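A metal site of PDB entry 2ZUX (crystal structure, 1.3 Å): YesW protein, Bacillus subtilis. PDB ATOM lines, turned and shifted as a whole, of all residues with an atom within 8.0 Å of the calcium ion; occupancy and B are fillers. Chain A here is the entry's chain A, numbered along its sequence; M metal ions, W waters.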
ATOM      1  N   GLY A 369      16.952 -15.416  22.192  1.00  0.00           N
ATOM      2  CA  GLY A 369      16.413 -14.739  23.372  1.00  0.00           C
ATOM      3  C   GLY A 369      17.510 -13.901  23.990  1.00  0.00           C
ATOM      4  O   GLY A 369      18.546 -13.667  23.372  1.00  0.00           O
ATOM      5  N   ASP A 370      17.275 -13.434  25.218  1.00  0.00           N
ATOM      6  CA  ASP A 370      18.336 -12.737  25.921  1.00  0.00           C
ATOM      7  C   ASP A 370      19.076 -13.794  26.716  1.00  0.00           C
ATOM      8  O   ASP A 370      18.734 -14.086  27.869  1.00  0.00           O
ATOM      9  CB  ASP A 370      17.838 -11.612  26.811  1.00  0.00           C
ATOM     10  CG  ASP A 370      18.973 -10.715  27.253  1.00  0.00           C
ATOM     11  OD1 ASP A 370      20.124 -11.000  26.849  1.00  0.00           O
ATOM     12  OD2 ASP A 370      18.740  -9.736  27.982  1.00  0.00           O
ATOM     13  N   LEU A 371      20.070 -14.392  26.062  1.00  0.00           N
ATOM     14  CA  LEU A 371      20.804 -15.512  26.618  1.00  0.00           C
ATOM     15  C   LEU A 371      21.925 -15.024  27.517  1.00  0.00           C
ATOM     16  O   LEU A 371      22.209 -15.616  28.564  1.00  0.00           O
ATOM     17  CB  LEU A 371      21.349 -16.402  25.490  1.00  0.00           C
ATOM     18  CG  LEU A 371      20.391 -16.827  24.359  1.00  0.00           C
ATOM     19  CD1 LEU A 371      21.070 -17.787  23.365  1.00  0.00           C
ATOM     20  CD2 LEU A 371      19.112 -17.453  24.920  1.00  0.00           C
ATOM     21  N   ASP A 372      22.563 -13.929  27.093  1.00  0.00           N
ATOM     22  CA  ASP A 372      23.587 -13.271  27.879  1.00  0.00           C
ATOM     23  C   ASP A 372      23.080 -11.888  28.275  1.00  0.00           C
ATOM     24  O   ASP A 372      23.195 -10.942  27.483  1.00  0.00           O
ATOM     25  CB  ASP A 372      24.895 -13.160  27.096  1.00  0.00           C
ATOM     26  CG  ASP A 372      26.025 -12.563  27.927  1.00  0.00           C
ATOM     27  OD1 ASP A 372      25.757 -12.096  29.051  1.00  0.00           O
ATOM     28  OD2 ASP A 372      27.178 -12.561  27.433  1.00  0.00           O
ATOM     29  N   PRO A 373      22.508 -11.755  29.486  1.00  0.00           N
ATOM     30  CA  PRO A 373      21.930 -10.481  29.900  1.00  0.00           C
ATOM     31  C   PRO A 373      22.988  -9.404  30.195  1.00  0.00           C
ATOM     32  O   PRO A 373      22.643  -8.226  30.332  1.00  0.00           O
ATOM     33  CB  PRO A 373      21.140 -10.862  31.163  1.00  0.00           C
ATOM     34  CG  PRO A 373      21.855 -12.024  31.717  1.00  0.00           C
ATOM     35  CD  PRO A 373      22.367 -12.798  30.525  1.00  0.00           C
ATOM     36  N   GLY A 374      24.267  -9.787  30.264  1.00  0.00           N
ATOM     37  CA  GLY A 374      25.359  -8.817  30.435  1.00  0.00           C
ATOM     38  C   GLY A 374      25.830  -8.188  29.134  1.00  0.00           C
ATOM     39  O   GLY A 374      26.601  -7.230  29.142  1.00  0.00           O
ATOM     40  N   ARG A 375      25.357  -8.731  28.016  1.00  0.00           N
ATOM     41  CA  ARG A 375      25.740  -8.234  26.705  1.00  0.00           C
ATOM     42  C   ARG A 375      24.499  -7.634  26.044  1.00  0.00           C
ATOM     43  O   ARG A 375      23.527  -8.342  25.807  1.00  0.00           O
ATOM     44  CB  ARG A 375      26.277  -9.380  25.851  1.00  0.00           C
ATOM     45  CG  ARG A 375      27.014  -8.943  24.594  1.00  0.00           C
ATOM     46  CD  ARG A 375      27.023 -10.038  23.540  1.00  0.00           C
ATOM     47  NE  ARG A 375      25.744 -10.107  22.857  1.00  0.00           N
ATOM     48  CZ  ARG A 375      25.447  -9.428  21.749  1.00  0.00           C
ATOM     49  NH1 ARG A 375      24.241  -9.535  21.209  1.00  0.00           N
ATOM     50  NH2 ARG A 375      26.357  -8.625  21.200  1.00  0.00           N
ATOM     51  N   PRO A 376      24.515  -6.313  25.758  1.00  0.00           N
ATOM     52  CA  PRO A 376      23.338  -5.700  25.130  1.00  0.00           C
ATOM     53  C   PRO A 376      22.924  -6.381  23.834  1.00  0.00           C
ATOM     54  O   PRO A 376      23.773  -6.705  23.003  1.00  0.00           O
ATOM     55  CB  PRO A 376      23.800  -4.260  24.861  1.00  0.00           C
ATOM     56  CG  PRO A 376      24.830  -4.009  25.885  1.00  0.00           C
ATOM     57  CD  PRO A 376      25.568  -5.312  26.010  1.00  0.00           C
ATOM     58  N   GLY A 377      21.619  -6.562  23.684  1.00  0.00           N
ATOM     59  CA  GLY A 377      21.057  -7.215  22.499  1.00  0.00           C
ATOM     60  C   GLY A 377      20.611  -8.645  22.791  1.00  0.00           C
ATOM     61  O   GLY A 377      20.761  -9.143  23.906  1.00  0.00           O
ATOM     62  N   LEU A 378      20.050  -9.294  21.776  1.00  0.00           N
ATOM     63  CA  LEU A 378      19.696 -10.702  21.883  1.00  0.00           C
ATOM     64  C   LEU A 378      20.816 -11.559  21.339  1.00  0.00           C
ATOM     65  O   LEU A 378      21.727 -11.071  20.664  1.00  0.00           O
ATOM     66  CB  LEU A 378      18.399 -10.978  21.126  1.00  0.00           C
ATOM     67  CG  LEU A 378      17.176 -10.196  21.598  1.00  0.00           C
ATOM     68  CD1 LEU A 378      15.972 -10.490  20.717  1.00  0.00           C
ATOM     69  CD2 LEU A 378      16.857 -10.486  23.060  1.00  0.00           C
ATOM     70  N   GLU A 379      20.764 -12.835  21.688  1.00  0.00           N
ATOM     71  CA  GLU A 379      21.764 -13.806  21.264  1.00  0.00           C
ATOM     72  C   GLU A 379      21.043 -15.000  20.655  1.00  0.00           C
ATOM     73  O   GLU A 379      19.874 -15.273  20.979  1.00  0.00           O
ATOM     74  CB  GLU A 379      22.654 -14.230  22.440  1.00  0.00           C
ATOM     75  CG  GLU A 379      23.582 -13.127  22.997  1.00  0.00           C
ATOM     76  CD  GLU A 379      22.890 -12.147  23.923  1.00  0.00           C
ATOM     77  OE1 GLU A 379      21.946 -12.527  24.655  1.00  0.00           O
ATOM     78  OE2 GLU A 379      23.320 -10.965  23.967  1.00  0.00           O
ATOM     79  N   PHE A 395      27.194 -19.558  19.152  1.00  0.00           N
ATOM     80  CA  PHE A 395      26.530 -18.612  20.033  1.00  0.00           C
ATOM     81  C   PHE A 395      26.879 -17.224  19.514  1.00  0.00           C
ATOM     82  O   PHE A 395      28.056 -16.845  19.494  1.00  0.00           O
ATOM     83  CB  PHE A 395      27.028 -18.825  21.467  1.00  0.00           C
ATOM     84  CG  PHE A 395      26.265 -18.057  22.525  1.00  0.00           C
ATOM     85  CD1 PHE A 395      25.345 -18.694  23.352  1.00  0.00           C
ATOM     86  CD2 PHE A 395      26.523 -16.704  22.737  1.00  0.00           C
ATOM     87  CE1 PHE A 395      24.663 -17.981  24.351  1.00  0.00           C
ATOM     88  CE2 PHE A 395      25.841 -15.991  23.714  1.00  0.00           C
ATOM     89  CZ  PHE A 395      24.908 -16.643  24.527  1.00  0.00           C
ATOM     90  N   LEU A 404      30.133 -15.012  18.939  1.00  0.00           N
ATOM     91  CA  LEU A 404      30.701 -14.675  20.244  1.00  0.00           C
ATOM     92  C   LEU A 404      31.581 -15.819  20.726  1.00  0.00           C
ATOM     93  O   LEU A 404      32.681 -15.600  21.232  1.00  0.00           O
ATOM     94  CB  LEU A 404      29.596 -14.333  21.246  1.00  0.00           C
ATOM     95  CG  LEU A 404      28.701 -13.200  20.742  1.00  0.00           C
ATOM     96  CD1 LEU A 404      27.438 -13.106  21.568  1.00  0.00           C
ATOM     97  CD2 LEU A 404      29.446 -11.872  20.761  1.00  0.00           C
ATOM     98  N   SER A 565      11.494 -12.049  25.313  1.00  0.00           N
ATOM     99  CA  SER A 565      12.311 -10.969  24.753  1.00  0.00           C
ATOM    100  C   SER A 565      13.315 -10.413  25.759  1.00  0.00           C
ATOM    101  O   SER A 565      14.283  -9.748  25.359  1.00  0.00           O
ATOM    102  CB  SER A 565      11.424  -9.831  24.271  1.00  0.00           C
ATOM    103  OG  SER A 565      10.793  -9.160  25.350  1.00  0.00           O
ATOM    104  N   PHE A 567      15.532 -11.197  29.637  1.00  0.00           N
ATOM    105  CA  PHE A 567      16.104 -12.263  30.420  1.00  0.00           C
ATOM    106  C   PHE A 567      15.200 -12.571  31.611  1.00  0.00           C
ATOM    107  O   PHE A 567      15.046 -11.743  32.511  1.00  0.00           O
ATOM    108  CB  PHE A 567      17.526 -11.939  30.903  1.00  0.00           C
ATOM    109  CG  PHE A 567      18.071 -12.944  31.866  1.00  0.00           C
ATOM    110  CD1 PHE A 567      18.394 -14.228  31.429  1.00  0.00           C
ATOM    111  CD2 PHE A 567      18.226 -12.624  33.212  1.00  0.00           C
ATOM    112  CE1 PHE A 567      18.863 -15.178  32.325  1.00  0.00           C
ATOM    113  CE2 PHE A 567      18.710 -13.578  34.113  1.00  0.00           C
ATOM    114  CZ  PHE A 567      19.029 -14.855  33.659  1.00  0.00           C
HETATM  115 CA    CA M   1      21.958 -10.002  25.740  1.00  0.00          CA
HETATM  116  O   HOH W   1      20.910  -8.281  27.113  1.00  0.00           O
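The backbone carbonyl oxygen (O) of Leu 378 is in hydrogen-bond range of the guanidinium group (NH1) of Arg 375 (3.0 Å). The backbone NH (N) of Gly 374 sits at hydrogen-bond distance from the side-chain carboxylate (OD1) of Asp 372. OE1 of Glu 379 lies close to N of Leu 371 (3.0 Å). N of Glu 379 lies within hydrogen-bond range of O of Gly 369, 2.9 Å away.
The calcium ion is bound by O of Arg 375 (2.3 Å), O of Asp 372 (2.3 Å), O of Gly 377 (2.4 Å), OD1 of Asp 370 (2.4 Å), OE2 of Glu 379 (2.4 Å), water W1 (2.4 Å) and OE1 of Glu 379 (2.7 Å). The calcium ion has seven donor atoms within binding distance.
Of the 15 residues printed, 5 come within 4 Å of the calcium ion. The nearest printed residue that does not touch the calcium ion is Pro 373 (4.2 Å).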
